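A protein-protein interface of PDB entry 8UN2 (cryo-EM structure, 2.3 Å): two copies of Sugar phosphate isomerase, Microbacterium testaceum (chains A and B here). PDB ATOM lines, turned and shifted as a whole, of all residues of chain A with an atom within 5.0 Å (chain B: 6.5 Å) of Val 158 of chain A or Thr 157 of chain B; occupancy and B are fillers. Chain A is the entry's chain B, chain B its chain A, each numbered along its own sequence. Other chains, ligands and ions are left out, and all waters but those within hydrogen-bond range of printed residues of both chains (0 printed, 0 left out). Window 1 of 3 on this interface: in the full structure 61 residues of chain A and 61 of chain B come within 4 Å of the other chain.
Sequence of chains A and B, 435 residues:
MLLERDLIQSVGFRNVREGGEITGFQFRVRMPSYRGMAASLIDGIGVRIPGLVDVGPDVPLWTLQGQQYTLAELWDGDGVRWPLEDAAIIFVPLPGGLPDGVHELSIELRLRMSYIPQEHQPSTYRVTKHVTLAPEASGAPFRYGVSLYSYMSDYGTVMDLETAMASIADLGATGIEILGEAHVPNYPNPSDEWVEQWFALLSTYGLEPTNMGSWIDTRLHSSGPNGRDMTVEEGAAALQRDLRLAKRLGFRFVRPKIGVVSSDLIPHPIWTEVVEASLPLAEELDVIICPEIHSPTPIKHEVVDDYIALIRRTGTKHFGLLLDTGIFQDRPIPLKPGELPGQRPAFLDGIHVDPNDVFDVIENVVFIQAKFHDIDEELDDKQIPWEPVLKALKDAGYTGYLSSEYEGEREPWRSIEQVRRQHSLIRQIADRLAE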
ATOM      1  N   LEU A   2     -18.832 -27.776  29.976  1.00  0.00           N
ATOM      2  CA  LEU A   2     -19.892 -26.889  29.542  1.00  0.00           C
ATOM      3  C   LEU A   2     -20.411 -27.308  28.172  1.00  0.00           C
ATOM      4  O   LEU A   2     -19.763 -28.050  27.435  1.00  0.00           O
ATOM      5  CB  LEU A   2     -19.385 -25.452  29.505  1.00  0.00           C
ATOM      6  CG  LEU A   2     -19.029 -24.872  30.870  1.00  0.00           C
ATOM      7  CD1 LEU A   2     -17.967 -23.821  30.727  1.00  0.00           C
ATOM      8  CD2 LEU A   2     -20.252 -24.286  31.530  1.00  0.00           C
ATOM      9  N   LEU A   3     -21.600 -26.825  27.840  1.00  0.00           N
ATOM     10  CA  LEU A   3     -22.254 -27.129  26.579  1.00  0.00           C
ATOM     11  C   LEU A   3     -22.466 -25.845  25.788  1.00  0.00           C
ATOM     12  O   LEU A   3     -22.178 -24.749  26.261  1.00  0.00           O
ATOM     13  CB  LEU A   3     -23.584 -27.847  26.825  1.00  0.00           C
ATOM     14  CG  LEU A   3     -23.452 -29.183  27.556  1.00  0.00           C
ATOM     15  CD1 LEU A   3     -24.753 -29.610  28.174  1.00  0.00           C
ATOM     16  CD2 LEU A   3     -22.962 -30.244  26.618  1.00  0.00           C
ATOM     17  N   GLU A   4     -22.956 -25.988  24.564  1.00  0.00           N
ATOM     18  CA  GLU A   4     -23.215 -24.845  23.704  1.00  0.00           C
ATOM     19  C   GLU A   4     -24.679 -24.433  23.794  1.00  0.00           C
ATOM     20  O   GLU A   4     -25.516 -25.177  24.300  1.00  0.00           O
ATOM     21  CB  GLU A   4     -22.845 -25.182  22.267  1.00  0.00           C
ATOM     22  CG  GLU A   4     -21.501 -25.859  22.146  1.00  0.00           C
ATOM     23  CD  GLU A   4     -21.287 -26.506  20.797  1.00  0.00           C
ATOM     24  OE1 GLU A   4     -20.771 -27.643  20.755  1.00  0.00           O
ATOM     25  OE2 GLU A   4     -21.633 -25.877  19.776  1.00  0.00           O
ATOM     26  N   ARG A   5     -24.993 -23.230  23.300  1.00  0.00           N
ATOM     27  CA  ARG A   5     -26.380 -22.770  23.357  1.00  0.00           C
ATOM     28  C   ARG A   5     -27.259 -23.512  22.371  1.00  0.00           C
ATOM     29  O   ARG A   5     -28.463 -23.666  22.605  1.00  0.00           O
ATOM     30  CB  ARG A   5     -26.498 -21.277  23.086  1.00  0.00           C
ATOM     31  CG  ARG A   5     -26.030 -20.438  24.184  1.00  0.00           C
ATOM     32  CD  ARG A   5     -26.831 -20.549  25.436  1.00  0.00           C
ATOM     33  NE  ARG A   5     -27.895 -19.567  25.500  1.00  0.00           N
ATOM     34  CZ  ARG A   5     -28.085 -18.780  26.550  1.00  0.00           C
ATOM     35  NH1 ARG A   5     -27.261 -18.849  27.580  1.00  0.00           N
ATOM     36  NH2 ARG A   5     -29.075 -17.912  26.561  1.00  0.00           N
ATOM     37  N   ARG A  30     -28.243 -31.078  23.687  1.00  0.00           N
ATOM     38  CA  ARG A  30     -28.466 -30.438  24.970  1.00  0.00           C
ATOM     39  C   ARG A  30     -29.939 -30.503  25.333  1.00  0.00           C
ATOM     40  O   ARG A  30     -30.813 -30.440  24.467  1.00  0.00           O
ATOM     41  CB  ARG A  30     -28.015 -28.985  24.918  1.00  0.00           C
ATOM     42  CG  ARG A  30     -27.676 -28.387  26.248  1.00  0.00           C
ATOM     43  CD  ARG A  30     -27.568 -26.893  26.145  1.00  0.00           C
ATOM     44  NE  ARG A  30     -28.776 -26.232  26.609  1.00  0.00           N
ATOM     45  CZ  ARG A  30     -29.306 -25.163  26.036  1.00  0.00           C
ATOM     46  NH1 ARG A  30     -28.740 -24.637  24.971  1.00  0.00           N
ATOM     47  NH2 ARG A  30     -30.409 -24.627  26.526  1.00  0.00           N
ATOM     48  N   ASP A 154     -13.608 -17.372  23.718  1.00  0.00           N
ATOM     49  CA  ASP A 154     -14.444 -18.433  24.260  1.00  0.00           C
ATOM     50  C   ASP A 154     -13.845 -19.013  25.529  1.00  0.00           C
ATOM     51  O   ASP A 154     -14.573 -19.350  26.467  1.00  0.00           O
ATOM     52  CB  ASP A 154     -14.637 -19.523  23.215  1.00  0.00           C
ATOM     53  CG  ASP A 154     -15.655 -19.148  22.169  1.00  0.00           C
ATOM     54  OD1 ASP A 154     -16.513 -18.296  22.458  1.00  0.00           O
ATOM     55  OD2 ASP A 154     -15.602 -19.704  21.056  1.00  0.00           O
ATOM     56  N   GLY A 156     -12.517 -19.086  29.002  1.00  0.00           N
ATOM     57  CA  GLY A 156     -12.703 -18.233  30.145  1.00  0.00           C
ATOM     58  C   GLY A 156     -14.082 -17.635  30.256  1.00  0.00           C
ATOM     59  O   GLY A 156     -14.453 -17.178  31.339  1.00  0.00           O
ATOM     60  N   THR A 157     -14.848 -17.617  29.172  1.00  0.00           N
ATOM     61  CA  THR A 157     -16.221 -17.141  29.196  1.00  0.00           C
ATOM     62  C   THR A 157     -17.227 -18.260  28.989  1.00  0.00           C
ATOM     63  O   THR A 157     -18.177 -18.379  29.762  1.00  0.00           O
ATOM     64  CB  THR A 157     -16.428 -16.056  28.134  1.00  0.00           C
ATOM     65  OG1 THR A 157     -16.138 -16.590  26.842  1.00  0.00           O
ATOM     66  CG2 THR A 157     -15.515 -14.895  28.390  1.00  0.00           C
ATOM     67  N   VAL A 158     -17.050 -19.086  27.961  1.00  0.00           N
ATOM     68  CA  VAL A 158     -17.938 -20.214  27.706  1.00  0.00           C
ATOM     69  C   VAL A 158     -17.230 -21.550  27.801  1.00  0.00           C
ATOM     70  O   VAL A 158     -17.879 -22.589  27.637  1.00  0.00           O
ATOM     71  CB  VAL A 158     -18.632 -20.097  26.333  1.00  0.00           C
ATOM     72  CG1 VAL A 158     -19.225 -18.747  26.150  1.00  0.00           C
ATOM     73  CG2 VAL A 158     -17.663 -20.379  25.219  1.00  0.00           C
ATOM     74  N   MET A 159     -15.933 -21.565  28.071  1.00  0.00           N
ATOM     75  CA  MET A 159     -15.144 -22.772  27.912  1.00  0.00           C
ATOM     76  C   MET A 159     -14.040 -22.804  28.952  1.00  0.00           C
ATOM     77  O   MET A 159     -13.451 -21.776  29.285  1.00  0.00           O
ATOM     78  CB  MET A 159     -14.549 -22.833  26.506  1.00  0.00           C
ATOM     79  CG  MET A 159     -14.162 -24.201  26.042  1.00  0.00           C
ATOM     80  SD  MET A 159     -13.426 -24.136  24.407  1.00  0.00           S
ATOM     81  CE  MET A 159     -14.718 -23.303  23.509  1.00  0.00           C
ATOM     82  N   ASP A 160     -13.762 -23.999  29.457  1.00  0.00           N
ATOM     83  CA  ASP A 160     -12.620 -24.248  30.319  1.00  0.00           C
ATOM     84  C   ASP A 160     -11.699 -25.246  29.633  1.00  0.00           C
ATOM     85  O   ASP A 160     -11.849 -25.541  28.449  1.00  0.00           O
ATOM     86  CB  ASP A 160     -13.043 -24.751  31.699  1.00  0.00           C
ATOM     87  CG  ASP A 160     -13.996 -25.907  31.629  1.00  0.00           C
ATOM     88  OD1 ASP A 160     -14.616 -26.090  30.573  1.00  0.00           O
ATOM     89  OD2 ASP A 160     -14.123 -26.643  32.626  1.00  0.00           O
ATOM     90  N   PRO A 412     -19.636 -15.802  19.949  1.00  0.00           N
ATOM     91  CA  PRO A 412     -19.617 -16.901  20.923  1.00  0.00           C
ATOM     92  C   PRO A 412     -20.027 -18.232  20.308  1.00  0.00           C
ATOM     93  O   PRO A 412     -21.010 -18.318  19.572  1.00  0.00           O
ATOM     94  CB  PRO A 412     -20.612 -16.437  21.987  1.00  0.00           C
ATOM     95  CG  PRO A 412     -20.610 -14.982  21.885  1.00  0.00           C
ATOM     96  CD  PRO A 412     -20.412 -14.658  20.448  1.00  0.00           C
ATOM     97  N   TRP A 413     -19.231 -19.263  20.598  1.00  0.00           N
ATOM     98  CA  TRP A 413     -19.274 -20.651  20.125  1.00  0.00           C
ATOM     99  C   TRP A 413     -19.025 -20.785  18.632  1.00  0.00           C
ATOM    100  O   TRP A 413     -19.195 -21.880  18.106  1.00  0.00           O
ATOM    101  CB  TRP A 413     -20.585 -21.380  20.450  1.00  0.00           C
ATOM    102  CG  TRP A 413     -20.800 -21.547  21.888  1.00  0.00           C
ATOM    103  CD1 TRP A 413     -20.314 -22.533  22.676  1.00  0.00           C
ATOM    104  CD2 TRP A 413     -21.549 -20.689  22.731  1.00  0.00           C
ATOM    105  NE1 TRP A 413     -20.718 -22.348  23.966  1.00  0.00           N
ATOM    106  CE2 TRP A 413     -21.481 -21.215  24.024  1.00  0.00           C
ATOM    107  CE3 TRP A 413     -22.281 -19.525  22.515  1.00  0.00           C
ATOM    108  CZ2 TRP A 413     -22.113 -20.621  25.094  1.00  0.00           C
ATOM    109  CZ3 TRP A 413     -22.887 -18.930  23.573  1.00  0.00           C
ATOM    110  CH2 TRP A 413     -22.795 -19.469  24.850  1.00  0.00           C
ATOM    111  N   LEU B   2     -16.217 -18.223  35.671  1.00  0.00           N
ATOM    112  CA  LEU B   2     -16.257 -17.735  34.307  1.00  0.00           C
ATOM    113  C   LEU B   2     -16.591 -16.248  34.283  1.00  0.00           C
ATOM    114  O   LEU B   2     -17.097 -15.684  35.251  1.00  0.00           O
ATOM    115  CB  LEU B   2     -17.280 -18.526  33.501  1.00  0.00           C
ATOM    116  CG  LEU B   2     -16.926 -19.996  33.298  1.00  0.00           C
ATOM    117  CD1 LEU B   2     -18.173 -20.815  33.138  1.00  0.00           C
ATOM    118  CD2 LEU B   2     -16.037 -20.164  32.091  1.00  0.00           C
ATOM    119  N   LEU B   3     -16.294 -15.616  33.156  1.00  0.00           N
ATOM    120  CA  LEU B   3     -16.532 -14.197  32.958  1.00  0.00           C
ATOM    121  C   LEU B   3     -17.508 -13.993  31.807  1.00  0.00           C
ATOM    122  O   LEU B   3     -17.914 -14.943  31.142  1.00  0.00           O
ATOM    123  CB  LEU B   3     -15.213 -13.465  32.694  1.00  0.00           C
ATOM    124  CG  LEU B   3     -14.200 -13.561  33.834  1.00  0.00           C
ATOM    125  CD1 LEU B   3     -12.805 -13.250  33.367  1.00  0.00           C
ATOM    126  CD2 LEU B   3     -14.581 -12.635  34.948  1.00  0.00           C
ATOM    127  N   ARG B   5     -18.749 -11.898  28.136  1.00  0.00           N
ATOM    128  CA  ARG B   5     -18.076 -11.465  26.912  1.00  0.00           C
ATOM    129  C   ARG B   5     -17.793  -9.976  26.922  1.00  0.00           C
ATOM    130  O   ARG B   5     -16.831  -9.521  26.296  1.00  0.00           O
ATOM    131  CB  ARG B   5     -18.886 -11.797  25.668  1.00  0.00           C
ATOM    132  CG  ARG B   5     -18.890 -13.216  25.327  1.00  0.00           C
ATOM    133  CD  ARG B   5     -17.561 -13.767  24.939  1.00  0.00           C
ATOM    134  NE  ARG B   5     -17.333 -13.705  23.509  1.00  0.00           N
ATOM    135  CZ  ARG B   5     -16.937 -14.749  22.799  1.00  0.00           C
ATOM    136  NH1 ARG B   5     -16.770 -15.920  23.387  1.00  0.00           N
ATOM    137  NH2 ARG B   5     -16.732 -14.635  21.502  1.00  0.00           N
ATOM    138  N   MET B 152     -31.505 -19.636  33.186  1.00  0.00           N
ATOM    139  CA  MET B 152     -32.020 -20.916  32.707  1.00  0.00           C
ATOM    140  C   MET B 152     -31.109 -21.525  31.652  1.00  0.00           C
ATOM    141  O   MET B 152     -30.590 -22.632  31.830  1.00  0.00           O
ATOM    142  CB  MET B 152     -33.433 -20.756  32.163  1.00  0.00           C
ATOM    143  CG  MET B 152     -33.943 -21.967  31.418  1.00  0.00           C
ATOM    144  SD  MET B 152     -35.567 -21.704  30.709  1.00  0.00           S
ATOM    145  CE  MET B 152     -35.600 -22.983  29.471  1.00  0.00           C
ATOM    146  N   SER B 153     -30.903 -20.828  30.544  1.00  0.00           N
ATOM    147  CA  SER B 153     -30.008 -21.350  29.528  1.00  0.00           C
ATOM    148  C   SER B 153     -28.563 -20.967  29.779  1.00  0.00           C
ATOM    149  O   SER B 153     -27.667 -21.544  29.159  1.00  0.00           O
ATOM    150  CB  SER B 153     -30.436 -20.867  28.145  1.00  0.00           C
ATOM    151  OG  SER B 153     -31.717 -21.362  27.817  1.00  0.00           O
ATOM    152  N   ASP B 154     -28.324 -20.018  30.681  1.00  0.00           N
ATOM    153  CA  ASP B 154     -26.961 -19.615  30.998  1.00  0.00           C
ATOM    154  C   ASP B 154     -26.263 -20.659  31.851  1.00  0.00           C
ATOM    155  O   ASP B 154     -25.067 -20.907  31.680  1.00  0.00           O
ATOM    156  CB  ASP B 154     -26.975 -18.267  31.708  1.00  0.00           C
ATOM    157  CG  ASP B 154     -27.178 -17.116  30.757  1.00  0.00           C
ATOM    158  OD1 ASP B 154     -26.875 -17.275  29.562  1.00  0.00           O
ATOM    159  OD2 ASP B 154     -27.640 -16.048  31.201  1.00  0.00           O
ATOM    160  N   TYR B 155     -26.992 -21.278  32.774  1.00  0.00           N
ATOM    161  CA  TYR B 155     -26.421 -22.304  33.633  1.00  0.00           C
ATOM    162  C   TYR B 155     -26.140 -23.559  32.827  1.00  0.00           C
ATOM    163  O   TYR B 155     -27.049 -24.147  32.239  1.00  0.00           O
ATOM    164  CB  TYR B 155     -27.374 -22.614  34.780  1.00  0.00           C
ATOM    165  CG  TYR B 155     -26.796 -23.472  35.864  1.00  0.00           C
ATOM    166  CD1 TYR B 155     -26.960 -24.846  35.842  1.00  0.00           C
ATOM    167  CD2 TYR B 155     -26.098 -22.909  36.916  1.00  0.00           C
ATOM    168  CE1 TYR B 155     -26.435 -25.634  36.822  1.00  0.00           C
ATOM    169  CE2 TYR B 155     -25.571 -23.693  37.908  1.00  0.00           C
ATOM    170  CZ  TYR B 155     -25.743 -25.055  37.853  1.00  0.00           C
ATOM    171  OH  TYR B 155     -25.221 -25.854  38.839  1.00  0.00           O
ATOM    172  N   GLY B 156     -24.882 -23.974  32.810  1.00  0.00           N
ATOM    173  CA  GLY B 156     -24.460 -25.123  32.050  1.00  0.00           C
ATOM    174  C   GLY B 156     -23.825 -24.791  30.726  1.00  0.00           C
ATOM    175  O   GLY B 156     -23.139 -25.644  30.158  1.00  0.00           O
ATOM    176  N   THR B 157     -24.036 -23.586  30.210  1.00  0.00           N
ATOM    177  CA  THR B 157     -23.401 -23.141  28.982  1.00  0.00           C
ATOM    178  C   THR B 157     -22.373 -22.049  29.222  1.00  0.00           C
ATOM    179  O   THR B 157     -21.247 -22.151  28.739  1.00  0.00           O
ATOM    180  CB  THR B 157     -24.454 -22.650  27.983  1.00  0.00           C
ATOM    181  OG1 THR B 157     -25.184 -21.565  28.556  1.00  0.00           O
ATOM    182  CG2 THR B 157     -25.414 -23.753  27.653  1.00  0.00           C
ATOM    183  N   VAL B 158     -22.730 -20.998  29.958  1.00  0.00           N
ATOM    184  CA  VAL B 158     -21.801 -19.921  30.278  1.00  0.00           C
ATOM    185  C   VAL B 158     -21.540 -19.796  31.765  1.00  0.00           C
ATOM    186  O   VAL B 158     -20.746 -18.940  32.168  1.00  0.00           O
ATOM    187  CB  VAL B 158     -22.285 -18.564  29.725  1.00  0.00           C
ATOM    188  CG1 VAL B 158     -22.678 -18.682  28.298  1.00  0.00           C
ATOM    189  CG2 VAL B 158     -23.444 -18.043  30.528  1.00  0.00           C
ATOM    190  N   MET B 159     -22.168 -20.620  32.594  1.00  0.00           N
ATOM    191  CA  MET B 159     -22.177 -20.386  34.024  1.00  0.00           C
ATOM    192  C   MET B 159     -22.195 -21.713  34.762  1.00  0.00           C
ATOM    193  O   MET B 159     -22.842 -22.667  34.332  1.00  0.00           O
ATOM    194  CB  MET B 159     -23.392 -19.548  34.415  1.00  0.00           C
ATOM    195  CG  MET B 159     -23.268 -18.819  35.715  1.00  0.00           C
ATOM    196  SD  MET B 159     -24.774 -17.919  36.089  1.00  0.00           S
ATOM    197  CE  MET B 159     -24.934 -16.936  34.615  1.00  0.00           C
ATOM    198  N   ASP B 160     -21.479 -21.760  35.877  1.00  0.00           N
ATOM    199  CA  ASP B 160     -21.530 -22.877  36.803  1.00  0.00           C
ATOM    200  C   ASP B 160     -22.049 -22.380  38.142  1.00  0.00           C
ATOM    201  O   ASP B 160     -22.554 -21.264  38.255  1.00  0.00           O
ATOM    202  CB  ASP B 160     -20.166 -23.551  36.959  1.00  0.00           C
ATOM    203  CG  ASP B 160     -19.067 -22.575  37.266  1.00  0.00           C
ATOM    204  OD1 ASP B 160     -19.256 -21.381  37.000  1.00  0.00           O
ATOM    205  OD2 ASP B 160     -18.015 -22.997  37.781  1.00  0.00           O
ATOM    206  N   TRP B 413     -25.893 -14.135  28.581  1.00  0.00           N
ATOM    207  CA  TRP B 413     -25.499 -13.186  29.629  1.00  0.00           C
ATOM    208  C   TRP B 413     -26.519 -12.084  29.857  1.00  0.00           C
ATOM    209  O   TRP B 413     -26.220 -11.152  30.597  1.00  0.00           O
ATOM    210  CB  TRP B 413     -24.136 -12.520  29.386  1.00  0.00           C
ATOM    211  CG  TRP B 413     -23.026 -13.474  29.413  1.00  0.00           C
ATOM    212  CD1 TRP B 413     -22.364 -13.924  30.501  1.00  0.00           C
ATOM    213  CD2 TRP B 413     -22.447 -14.120  28.291  1.00  0.00           C
ATOM    214  NE1 TRP B 413     -21.397 -14.814  30.131  1.00  0.00           N
ATOM    215  CE2 TRP B 413     -21.430 -14.949  28.772  1.00  0.00           C
ATOM    216  CE3 TRP B 413     -22.686 -14.070  26.921  1.00  0.00           C
ATOM    217  CZ2 TRP B 413     -20.657 -15.723  27.935  1.00  0.00           C
ATOM    218  CZ3 TRP B 413     -21.935 -14.846  26.099  1.00  0.00           C
ATOM    219  CH2 TRP B 413     -20.938 -15.670  26.604  1.00  0.00           C
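Hydrophobic or aromatic side chains of chain B that line the printed part of chain A: Leu 2, Val 158 and Trp 413.
Among the printed residues, 21 pairs touch across the chains.
O of Asp 154 of chain B sits at hydrogen-bond distance from OG1 of Thr 157 of chain B, 3.2 Å away.
N of Met 159 of chain B lies within hydrogen-bond range of O of Asp 154 of chain B.
OD1 of Asp 154 of chain B is in hydrogen-bond range of N of Trp 413 of chain B, at 3.4 Å.
The backbone carbonyl oxygen of Arg 5 of chain A lies within hydrogen-bond range of the guanidinium group of Arg 30 of chain A (2.6 Å).
The side-chain hydroxyl of Thr 157 of chain A lies within hydrogen-bond range of the backbone carbonyl oxygen of Asp 154 of chain A (3.2 Å).
The backbone NH (N) of Trp 413 of chain A sits at hydrogen-bond distance from the side-chain carboxylate (OD1) of Asp 154 of chain A (3.4 Å).
Of the printed residues of chain B, Glu 4 of chain A touches Thr 157.
Of chain B, only Thr 157 and Trp 413 come within 4 Å of Val 158 of chain A.
Of the printed residues of chain B, Trp 413 of chain A touches Val 158 (3.5 Å).
Thr 157 of chain B touches just these residues of chain A: Leu 2 (3.7 Å), Leu 3 (3.4 Å), Glu 4 (3.6 Å), Arg 5 (3.6 Å) and Val 158 (3.6 Å).
Printed residues of chain A within 4 Å of Trp 413 of chain B: Val 158 (3.6 Å).
The nearest residue of chain A that does not touch Thr 157 of chain B is Trp 413 of chain A (4.05 Å).
Leu 2 of chain A touches Gly 156 of chain B, and with the chains exchanged Gly 156 of chain A touches Leu 2 of chain B.
Leu 2 of chain A touches Thr 157 of chain B, and with the chains exchanged Thr 157 of chain A touches Leu 2 of chain B.
Leu 3 of chain A touches Thr 157 of chain B, and with the chains exchanged Thr 157 of chain A touches Leu 3 of chain B.
Val 158 of chain A touches Trp 413 of chain B, and with the chains exchanged Trp 413 of chain A touches Val 158 of chain B.
Leu 2 of chain A touches Gly 156 of chain B.
O of Thr 157 of chain B touches CD2 of Leu 2 of chain A (3.7 Å).
Leu 3 of chain A touches Thr 157 of chain B.
Glu 4 of chain A touches Thr 157 of chain B (O to CG2, 3.6 Å).
Arg 5 of chain A touches Thr 157 of chain B.
O of Gly 156 of chain A touches CD2 of Leu 2 of chain B (3.5 Å).
OG1 of Thr 157 of chain A touches NH1 of Arg 5 of chain B, at 3.6 Å.
Thr 157 of chain B touches Val 158 of chain A.
CG1 of Val 158 of chain A touches CH2 of Trp 413 of chain B, 3.6 Å away.
Val 158 of chain B touches Trp 413 of chain A (CG1 to CH2, 3.5 Å).
The backbone NH (N) of Leu 3 of chain B sits at hydrogen-bond distance from the backbone carbonyl oxygen (O) of Gly 156 of chain A, at 3.0 Å.
The side-chain carboxylate (OD1) of Asp 154 of chain A lies within salt-bridge range of the guanidinium group (NH1) of Arg 5 of chain B (2.6 Å).
The guanidinium group of Arg 5 of chain A sits at hydrogen-bond distance from the backbone carbonyl oxygen of Ser 153 of chain B (3.1 Å).
The guanidinium group (NH1) of Arg 5 of chain A is in salt-bridge range of the side-chain carboxylate (OD1) of Asp 154 of chain B (2.6 Å).
The backbone NH of Leu 3 of chain A is in hydrogen-bond range of the backbone carbonyl oxygen of Gly 156 of chain B (3.0 Å).
The guanidinium group (NH2) of Arg 5 of chain B sits close to the backbone nitrogen (N) of Pro 412 of chain A (3.5 Å).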
